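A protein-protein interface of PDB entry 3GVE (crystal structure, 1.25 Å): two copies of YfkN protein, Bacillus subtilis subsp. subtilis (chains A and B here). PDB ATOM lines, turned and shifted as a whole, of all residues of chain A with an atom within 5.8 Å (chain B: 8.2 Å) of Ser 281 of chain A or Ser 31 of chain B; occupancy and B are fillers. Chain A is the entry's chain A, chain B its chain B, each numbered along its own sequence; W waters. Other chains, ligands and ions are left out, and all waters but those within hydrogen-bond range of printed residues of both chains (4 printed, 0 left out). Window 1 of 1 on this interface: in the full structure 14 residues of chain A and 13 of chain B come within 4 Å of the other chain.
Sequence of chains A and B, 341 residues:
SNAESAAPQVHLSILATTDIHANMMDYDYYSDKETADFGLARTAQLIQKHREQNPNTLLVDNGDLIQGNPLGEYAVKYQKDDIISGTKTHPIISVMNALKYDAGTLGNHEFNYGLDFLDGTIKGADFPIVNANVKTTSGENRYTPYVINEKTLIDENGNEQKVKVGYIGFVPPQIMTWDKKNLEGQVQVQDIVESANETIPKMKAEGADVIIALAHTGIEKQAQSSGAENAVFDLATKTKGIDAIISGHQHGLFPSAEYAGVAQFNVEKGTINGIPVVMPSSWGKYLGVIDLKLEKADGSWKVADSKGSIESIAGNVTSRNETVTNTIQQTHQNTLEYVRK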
ATOM      1  N   THR A  18      28.261  -8.964 -30.656  1.00  0.00           N
ATOM      2  CA  THR A  18      26.876  -8.543 -30.516  1.00  0.00           C
ATOM      3  C   THR A  18      26.752  -7.408 -29.514  1.00  0.00           C
ATOM      4  O   THR A  18      27.528  -7.312 -28.584  1.00  0.00           O
ATOM      5  CB  THR A  18      25.942  -9.725 -30.076  1.00  0.00           C
ATOM      6  OG1 THR A  18      24.563  -9.388 -30.327  1.00  0.00           O
ATOM      7  CG2 THR A  18      26.135 -10.083 -28.593  1.00  0.00           C
ATOM      8  N   ASP A  19      25.740  -6.579 -29.705  1.00  0.00           N
ATOM      9  CA  ASP A  19      25.400  -5.536 -28.744  1.00  0.00           C
ATOM     10  C   ASP A  19      26.615  -4.668 -28.366  1.00  0.00           C
ATOM     11  O   ASP A  19      26.803  -4.281 -27.233  1.00  0.00           O
ATOM     12  CB  ASP A  19      24.694  -6.139 -27.511  1.00  0.00           C
ATOM     13  CG  ASP A  19      23.336  -6.723 -27.859  1.00  0.00           C
ATOM     14  OD1 ASP A  19      22.337  -5.977 -27.778  1.00  0.00           O
ATOM     15  OD2 ASP A  19      23.280  -7.921 -28.218  1.00  0.00           O
ATOM     16  N   GLY A 248      21.900 -12.591 -29.244  1.00  0.00           N
ATOM     17  CA  GLY A 248      22.198 -11.344 -28.544  1.00  0.00           C
ATOM     18  C   GLY A 248      20.965 -10.826 -27.803  1.00  0.00           C
ATOM     19  O   GLY A 248      20.189 -11.605 -27.281  1.00  0.00           O
ATOM     20  N   HIS A 251      21.980  -9.347 -23.566  1.00  0.00           N
ATOM     21  CA  HIS A 251      23.220  -8.938 -22.900  1.00  0.00           C
ATOM     22  C   HIS A 251      23.684  -9.997 -21.867  1.00  0.00           C
ATOM     23  O   HIS A 251      24.406  -9.679 -20.932  1.00  0.00           O
ATOM     24  CB  HIS A 251      23.096  -7.529 -22.256  1.00  0.00           C
ATOM     25  CG  HIS A 251      22.893  -6.401 -23.235  1.00  0.00           C
ATOM     26  ND1 HIS A 251      23.158  -5.093 -22.905  1.00  0.00           N
ATOM     27  CD2 HIS A 251      22.438  -6.376 -24.514  1.00  0.00           C
ATOM     28  CE1 HIS A 251      22.902  -4.313 -23.942  1.00  0.00           C
ATOM     29  NE2 HIS A 251      22.442  -5.063 -24.925  1.00  0.00           N
ATOM     30  N   GLY A 252      23.275 -11.250 -22.071  1.00  0.00           N
ATOM     31  CA  GLY A 252      23.683 -12.375 -21.236  1.00  0.00           C
ATOM     32  C   GLY A 252      24.824 -13.189 -21.820  1.00  0.00           C
ATOM     33  O   GLY A 252      25.455 -12.746 -22.773  1.00  0.00           O
ATOM     34  N   LEU A 253      25.079 -14.371 -21.246  1.00  0.00           N
ATOM     35  CA  LEU A 253      26.136 -15.247 -21.699  1.00  0.00           C
ATOM     36  C   LEU A 253      25.541 -16.558 -22.153  1.00  0.00           C
ATOM     37  O   LEU A 253      24.705 -17.148 -21.430  1.00  0.00           O
ATOM     38  CB  LEU A 253      27.151 -15.530 -20.557  1.00  0.00           C
ATOM     39  CG  LEU A 253      27.814 -14.299 -19.931  1.00  0.00           C
ATOM     40  CD1 LEU A 253      28.878 -14.776 -18.887  1.00  0.00           C
ATOM     41  CD2 LEU A 253      28.437 -13.425 -20.937  1.00  0.00           C
ATOM     42  N   MET A 279      26.209 -16.382 -27.368  1.00  0.00           N
ATOM     43  CA  MET A 279      25.743 -15.050 -26.990  1.00  0.00           C
ATOM     44  C   MET A 279      26.870 -14.394 -26.200  1.00  0.00           C
ATOM     45  O   MET A 279      27.050 -14.644 -25.008  1.00  0.00           O
ATOM     46  CB  MET A 279      24.464 -15.099 -26.143  1.00  0.00           C
ATOM     47  CG  MET A 279      23.993 -13.705 -25.702  1.00  0.00           C
ATOM     48  SD  MET A 279      22.568 -13.763 -24.387  1.00  0.00           S
ATOM     49  CE  MET A 279      21.159 -14.467 -25.493  1.00  0.00           C
ATOM     50  N   PRO A 280      27.634 -13.562 -26.887  1.00  0.00           N
ATOM     51  CA  PRO A 280      28.835 -12.986 -26.276  1.00  0.00           C
ATOM     52  C   PRO A 280      28.612 -11.647 -25.577  1.00  0.00           C
ATOM     53  O   PRO A 280      29.210 -10.650 -25.900  1.00  0.00           O
ATOM     54  CB  PRO A 280      29.787 -12.847 -27.464  1.00  0.00           C
ATOM     55  CG  PRO A 280      28.892 -12.598 -28.615  1.00  0.00           C
ATOM     56  CD  PRO A 280      27.678 -13.468 -28.361  1.00  0.00           C
ATOM     57  N   SER A 281      27.764 -11.663 -24.567  1.00  0.00           N
ATOM     58  CA  SER A 281      27.612 -10.544 -23.634  1.00  0.00           C
ATOM     59  C   SER A 281      27.179  -9.267 -24.377  1.00  0.00           C
ATOM     60  O   SER A 281      26.298  -9.305 -25.216  1.00  0.00           O
ATOM     61  CB  SER A 281      28.930 -10.351 -22.844  1.00  0.00           C
ATOM     62  OG  SER A 281      28.740  -9.435 -21.774  1.00  0.00           O
ATOM     63  N   SER A 282      27.778  -8.143 -24.021  1.00  0.00           N
ATOM     64  CA  SER A 282      27.491  -6.868 -24.663  1.00  0.00           C
ATOM     65  C   SER A 282      28.759  -6.013 -24.628  1.00  0.00           C
ATOM     66  O   SER A 282      29.693  -6.314 -23.913  1.00  0.00           O
ATOM     67  CB  SER A 282      26.319  -6.159 -23.986  1.00  0.00           C
ATOM     68  OG  SER A 282      26.644  -5.824 -22.657  1.00  0.00           O
ATOM     69  N   TRP A 283      28.781  -4.981 -25.458  1.00  0.00           N
ATOM     70  CA  TRP A 283      29.831  -3.955 -25.481  1.00  0.00           C
ATOM     71  C   TRP A 283      31.227  -4.477 -25.834  1.00  0.00           C
ATOM     72  O   TRP A 283      32.219  -3.829 -25.558  1.00  0.00           O
ATOM     73  CB  TRP A 283      29.873  -3.192 -24.139  1.00  0.00           C
ATOM     74  CG  TRP A 283      28.658  -2.382 -23.829  1.00  0.00           C
ATOM     75  CD1 TRP A 283      27.443  -2.462 -24.395  1.00  0.00           C
ATOM     76  CD2 TRP A 283      28.578  -1.353 -22.837  1.00  0.00           C
ATOM     77  NE1 TRP A 283      26.589  -1.534 -23.823  1.00  0.00           N
ATOM     78  CE2 TRP A 283      27.271  -0.843 -22.861  1.00  0.00           C
ATOM     79  CE3 TRP A 283      29.494  -0.821 -21.931  1.00  0.00           C
ATOM     80  CZ2 TRP A 283      26.849   0.192 -22.014  1.00  0.00           C
ATOM     81  CZ3 TRP A 283      29.079   0.202 -21.096  1.00  0.00           C
ATOM     82  CH2 TRP A 283      27.770   0.696 -21.148  1.00  0.00           C
ATOM     83  N   LYS A 285      32.551  -7.265 -24.563  1.00  0.00           N
ATOM     84  CA  LYS A 285      33.158  -7.934 -23.402  1.00  0.00           C
ATOM     85  C   LYS A 285      33.569  -9.400 -23.632  1.00  0.00           C
ATOM     86  O   LYS A 285      34.407  -9.932 -22.928  1.00  0.00           O
ATOM     87  CB  LYS A 285      32.241  -7.815 -22.175  1.00  0.00           C
ATOM     88  CG  LYS A 285      32.089  -6.371 -21.656  1.00  0.00           C
ATOM     89  CD  LYS A 285      31.006  -6.266 -20.577  1.00  0.00           C
ATOM     90  CE  LYS A 285      30.805  -4.829 -20.086  1.00  0.00           C
ATOM     91  NZ  LYS A 285      29.738  -4.811 -19.045  1.00  0.00           N
ATOM     92  N   TYR A 286      32.966 -10.020 -24.637  1.00  0.00           N
ATOM     93  CA  TYR A 286      33.256 -11.390 -25.034  1.00  0.00           C
ATOM     94  C   TYR A 286      33.217 -11.453 -26.559  1.00  0.00           C
ATOM     95  O   TYR A 286      32.560 -10.635 -27.196  1.00  0.00           O
ATOM     96  CB  TYR A 286      32.194 -12.338 -24.485  1.00  0.00           C
ATOM     97  CG  TYR A 286      32.331 -12.703 -23.030  1.00  0.00           C
ATOM     98  CD1 TYR A 286      32.775 -13.957 -22.660  1.00  0.00           C
ATOM     99  CD2 TYR A 286      31.989 -11.810 -22.036  1.00  0.00           C
ATOM    100  CE1 TYR A 286      32.889 -14.312 -21.316  1.00  0.00           C
ATOM    101  CE2 TYR A 286      32.102 -12.157 -20.695  1.00  0.00           C
ATOM    102  CZ  TYR A 286      32.550 -13.401 -20.355  1.00  0.00           C
ATOM    103  OH  TYR A 286      32.662 -13.742 -19.024  1.00  0.00           O
ATOM    104  N   ILE A 310      32.329 -18.953 -25.748  1.00  0.00           N
ATOM    105  CA  ILE A 310      32.570 -17.522 -25.710  1.00  0.00           C
ATOM    106  C   ILE A 310      33.868 -17.314 -24.958  1.00  0.00           C
ATOM    107  O   ILE A 310      34.217 -18.098 -24.108  1.00  0.00           O
ATOM    108  CB  ILE A 310      31.414 -16.742 -25.060  1.00  0.00           C
ATOM    109  CG1 ILE A 310      31.073 -17.333 -23.677  1.00  0.00           C
ATOM    110  CG2 ILE A 310      30.169 -16.759 -25.969  1.00  0.00           C
ATOM    111  CD1 ILE A 310      30.023 -16.541 -22.917  1.00  0.00           C
ATOM    112  N   TYR B  27      27.491  -6.577  -8.541  1.00  0.00           N
ATOM    113  CA  TYR B  27      27.017  -7.719  -9.301  1.00  0.00           C
ATOM    114  C   TYR B  27      26.330  -7.284 -10.582  1.00  0.00           C
ATOM    115  O   TYR B  27      25.531  -6.356 -10.578  1.00  0.00           O
ATOM    116  CB  TYR B  27      26.046  -8.541  -8.436  1.00  0.00           C
ATOM    117  CG  TYR B  27      25.922  -9.984  -8.889  1.00  0.00           C
ATOM    118  CD1 TYR B  27      26.817 -10.949  -8.442  1.00  0.00           C
ATOM    119  CD2 TYR B  27      24.929 -10.373  -9.775  1.00  0.00           C
ATOM    120  CE1 TYR B  27      26.719 -12.252  -8.859  1.00  0.00           C
ATOM    121  CE2 TYR B  27      24.825 -11.690 -10.191  1.00  0.00           C
ATOM    122  CZ  TYR B  27      25.731 -12.611  -9.719  1.00  0.00           C
ATOM    123  OH  TYR B  27      25.673 -13.924 -10.116  1.00  0.00           O
ATOM    124  N   ASP B  28      26.655  -7.978 -11.669  1.00  0.00           N
ATOM    125  CA  ASP B  28      26.044  -7.796 -12.974  1.00  0.00           C
ATOM    126  C   ASP B  28      25.037  -8.936 -13.183  1.00  0.00           C
ATOM    127  O   ASP B  28      25.434 -10.075 -13.388  1.00  0.00           O
ATOM    128  CB  ASP B  28      27.149  -7.841 -14.044  1.00  0.00           C
ATOM    129  CG  ASP B  28      26.620  -7.779 -15.466  1.00  0.00           C
ATOM    130  OD1 ASP B  28      25.421  -7.650 -15.672  1.00  0.00           O
ATOM    131  OD2 ASP B  28      27.444  -7.895 -16.385  1.00  0.00           O
ATOM    132  N   TYR B  29      23.746  -8.644 -13.097  1.00  0.00           N
ATOM    133  CA  TYR B  29      22.719  -9.667 -13.212  1.00  0.00           C
ATOM    134  C   TYR B  29      22.577 -10.170 -14.643  1.00  0.00           C
ATOM    135  O   TYR B  29      22.055 -11.242 -14.847  1.00  0.00           O
ATOM    136  CB  TYR B  29      21.355  -9.165 -12.723  1.00  0.00           C
ATOM    137  CG  TYR B  29      21.286  -8.889 -11.223  1.00  0.00           C
ATOM    138  CD1 TYR B  29      21.225  -9.928 -10.293  1.00  0.00           C
ATOM    139  CD2 TYR B  29      21.298  -7.589 -10.742  1.00  0.00           C
ATOM    140  CE1 TYR B  29      21.181  -9.670  -8.941  1.00  0.00           C
ATOM    141  CE2 TYR B  29      21.242  -7.333  -9.394  1.00  0.00           C
ATOM    142  CZ  TYR B  29      21.176  -8.372  -8.503  1.00  0.00           C
ATOM    143  OH  TYR B  29      21.125  -8.119  -7.162  1.00  0.00           O
ATOM    144  N   TYR B  30      23.036  -9.380 -15.607  1.00  0.00           N
ATOM    145  CA  TYR B  30      22.930  -9.753 -17.020  1.00  0.00           C
ATOM    146  C   TYR B  30      23.961 -10.808 -17.392  1.00  0.00           C
ATOM    147  O   TYR B  30      23.563 -11.818 -17.930  1.00  0.00           O
ATOM    148  CB  TYR B  30      23.021  -8.532 -17.948  1.00  0.00           C
ATOM    149  CG  TYR B  30      22.145  -7.386 -17.490  1.00  0.00           C
ATOM    150  CD1 TYR B  30      20.764  -7.492 -17.473  1.00  0.00           C
ATOM    151  CD2 TYR B  30      22.712  -6.213 -17.056  1.00  0.00           C
ATOM    152  CE1 TYR B  30      19.973  -6.441 -17.025  1.00  0.00           C
ATOM    153  CE2 TYR B  30      21.941  -5.166 -16.616  1.00  0.00           C
ATOM    154  CZ  TYR B  30      20.584  -5.279 -16.603  1.00  0.00           C
ATOM    155  OH  TYR B  30      19.853  -4.201 -16.158  1.00  0.00           O
ATOM    156  N   SER B  31      25.238 -10.660 -17.063  1.00  0.00           N
ATOM    157  CA  SER B  31      26.230 -11.694 -17.260  1.00  0.00           C
ATOM    158  C   SER B  31      26.112 -12.715 -16.152  1.00  0.00           C
ATOM    159  O   SER B  31      26.685 -13.783 -16.232  1.00  0.00           O
ATOM    160  CB  SER B  31      27.617 -11.087 -17.173  1.00  0.00           C
ATOM    161  OG  SER B  31      27.721  -9.940 -17.974  1.00  0.00           O
ATOM    162  N   ASP B  32      25.419 -12.461 -15.075  1.00  0.00           N
ATOM    163  CA  ASP B  32      25.259 -13.265 -13.872  1.00  0.00           C
ATOM    164  C   ASP B  32      26.620 -13.503 -13.240  1.00  0.00           C
ATOM    165  O   ASP B  32      27.020 -14.622 -12.996  1.00  0.00           O
ATOM    166  CB  ASP B  32      24.547 -14.581 -14.201  1.00  0.00           C
ATOM    167  CG  ASP B  32      23.911 -15.250 -12.985  1.00  0.00           C
ATOM    168  OD1 ASP B  32      23.962 -14.715 -11.887  1.00  0.00           O
ATOM    169  OD2 ASP B  32      23.335 -16.335 -13.166  1.00  0.00           O
ATOM    170  N   LYS B  33      27.326 -12.419 -12.961  1.00  0.00           N
ATOM    171  CA  LYS B  33      28.682 -12.464 -12.422  1.00  0.00           C
ATOM    172  C   LYS B  33      28.942 -11.282 -11.503  1.00  0.00           C
ATOM    173  O   LYS B  33      28.432 -10.201 -11.726  1.00  0.00           O
ATOM    174  CB  LYS B  33      29.711 -12.360 -13.556  1.00  0.00           C
ATOM    175  CG  LYS B  33      29.749 -13.517 -14.491  1.00  0.00           C
ATOM    176  CD  LYS B  33      30.818 -13.288 -15.500  1.00  0.00           C
ATOM    177  CE  LYS B  33      31.408 -14.596 -15.955  1.00  0.00           C
ATOM    178  NZ  LYS B  33      32.323 -15.183 -14.950  1.00  0.00           N
ATOM    179  N   GLU B  34      29.770 -11.513 -10.502  1.00  0.00           N
ATOM    180  CA  GLU B  34      30.367 -10.498  -9.676  1.00  0.00           C
ATOM    181  C   GLU B  34      31.219  -9.512 -10.481  1.00  0.00           C
ATOM    182  O   GLU B  34      31.884  -9.878 -11.426  1.00  0.00           O
ATOM    183  CB  GLU B  34      31.256 -11.227  -8.670  1.00  0.00           C
ATOM    184  CG  GLU B  34      31.885 -10.409  -7.632  1.00  0.00           C
ATOM    185  CD  GLU B  34      32.685 -11.254  -6.645  1.00  0.00           C
ATOM    186  OE1 GLU B  34      33.040 -12.409  -6.949  1.00  0.00           O
ATOM    187  OE2 GLU B  34      32.938 -10.755  -5.555  1.00  0.00           O
ATOM    188  N   VAL B 339      15.948 -13.943 -12.290  1.00  0.00           N
ATOM    189  CA  VAL B 339      16.679 -13.743 -13.526  1.00  0.00           C
ATOM    190  C   VAL B 339      17.000 -15.049 -14.254  1.00  0.00           C
ATOM    191  O   VAL B 339      17.039 -15.078 -15.480  1.00  0.00           O
ATOM    192  CB  VAL B 339      18.000 -12.971 -13.267  1.00  0.00           C
ATOM    193  CG1 VAL B 339      18.826 -12.936 -14.485  1.00  0.00           C
ATOM    194  CG2 VAL B 339      17.701 -11.545 -12.780  1.00  0.00           C
ATOM    195  N   ARG B 340      17.246 -16.097 -13.477  1.00  0.00           N
ATOM    196  CA  ARG B 340      17.736 -17.373 -13.998  1.00  0.00           C
ATOM    197  C   ARG B 340      16.611 -18.195 -14.559  1.00  0.00           C
ATOM    198  O   ARG B 340      16.835 -19.198 -15.226  1.00  0.00           O
ATOM    199  CB  ARG B 340      18.481 -18.146 -12.917  1.00  0.00           C
ATOM    200  CG  ARG B 340      19.933 -17.722 -12.794  1.00  0.00           C
ATOM    201  CD  ARG B 340      20.472 -17.999 -11.458  1.00  0.00           C
ATOM    202  NE  ARG B 340      21.809 -17.458 -11.272  1.00  0.00           N
ATOM    203  CZ  ARG B 340      22.494 -17.646 -10.154  1.00  0.00           C
ATOM    204  NH1 ARG B 340      21.959 -18.369  -9.178  1.00  0.00           N
ATOM    205  NH2 ARG B 340      23.707 -17.131 -10.009  1.00  0.00           N
HETATM  206  O   HOH W   1      27.227  -6.624 -18.625  1.00  0.00           O
HETATM  207  O   HOH W   2      23.875 -14.706 -18.548  1.00  0.00           O
HETATM  208  O   HOH W   3      32.995 -16.072 -18.136  1.00  0.00           O
HETATM  209  O   HOH W   4      30.068  -9.644 -19.554  1.00  0.00           O
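The backbone carbonyl oxygen (O) of Gly 252 of chain A is in hydrogen-bond range of the backbone NH (N) of Ser 281 of chain A (3.1 Å).
The side-chain carboxylate of Asp 28 of chain B sits at hydrogen-bond distance from the side-chain hydroxyl of Ser 31 of chain B, 2.6 Å away.
OD1 of Asp 28 of chain B sits at hydrogen-bond distance from N of Tyr 30 of chain B (2.9 Å).
The backbone NH (N) of Gly 252 of chain A sits close to the side-chain sulfur (SD) of Met 279 of chain A (3.5 Å).
The backbone carbonyl oxygen of Lys 33 of chain B is in hydrogen-bond range of the backbone NH of Asp 28 of chain B (2.8 Å).
O of His 251 of chain A touches CB of Tyr 30 of chain B, 3.5 Å away.
CA of Gly 252 of chain A touches O of Tyr 30 of chain B, 3.4 Å away.
O of Ser 31 of chain B touches CD1 of Leu 253 of chain A (3.6 Å).
CD1 of Leu 253 of chain A touches CE of Lys 33 of chain B (3.9 Å).
Ser 281 of chain A touches Ser 31 of chain B.
Tyr 286 of chain A touches Lys 33 of chain B.
Of the printed residues of chain B, His 251 of chain A touches Tyr 30.
Printed residues of chain B within 4 Å of Gly 252 of chain A: Tyr 30 (3.4 Å).
Of the printed residues of chain B, Leu 253 of chain A touches Ser 31 (3.6 Å) and Lys 33 (3.9 Å).
Printed residues of chain B within 4 Å of Ser 281 of chain A: Ser 31 (3.97 Å).
No residue of chain B comes within 4 Å of Ser 282 of chain A.
Of the printed residues of chain B, Tyr 286 of chain A touches Lys 33 (3.4 Å).
Of the printed residues of chain A, Ser 31 of chain B touches Leu 253 and Ser 281.
Of the printed residues of chain A, Lys 33 of chain B touches Leu 253 (3.9 Å) and Tyr 286 (3.4 Å).
Val 339 of chain B touches none of the printed residues of chain A.
The nearest printed residue of chain B that does not touch Ser 281 of chain A is Asp 28 of chain B (5.8 Å).
The nearest printed residue of chain A that does not touch Ser 31 of chain B is His 251 of chain A (4.1 Å).
Of the 14 printed residues of chain A, 5 touch a printed residue of chain B.
Printed residues of chain B that touch a printed residue of chain A: Tyr 30, Ser 31 and Lys 33.
No position is printed for both chains.
Of the 6 pairs that touch across the chains among the printed residues, none has its exchanged pair printed and touching as well.
Water W3 lies within hydrogen-bond range of OH of Tyr 286 of chain A (2.5 Å) and NZ of Lys 33 of chain B (3.4 Å).
Water W1 lies within hydrogen-bond range of OD2 of Asp 28 of chain B (2.6 Å), NZ of Lys 285 of chain A (3.1 Å) and OG of Ser 31 of chain B (3.4 Å).
Water W4 bridges the side-chain hydroxyl of Ser 281 of chain A (2.6 Å) and the side-chain hydroxyl of Ser 31 of chain B (2.8 Å).
Water W2 bridges O of Tyr 30 of chain B (3.0 Å) and N of Leu 253 of chain A (3.0 Å).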
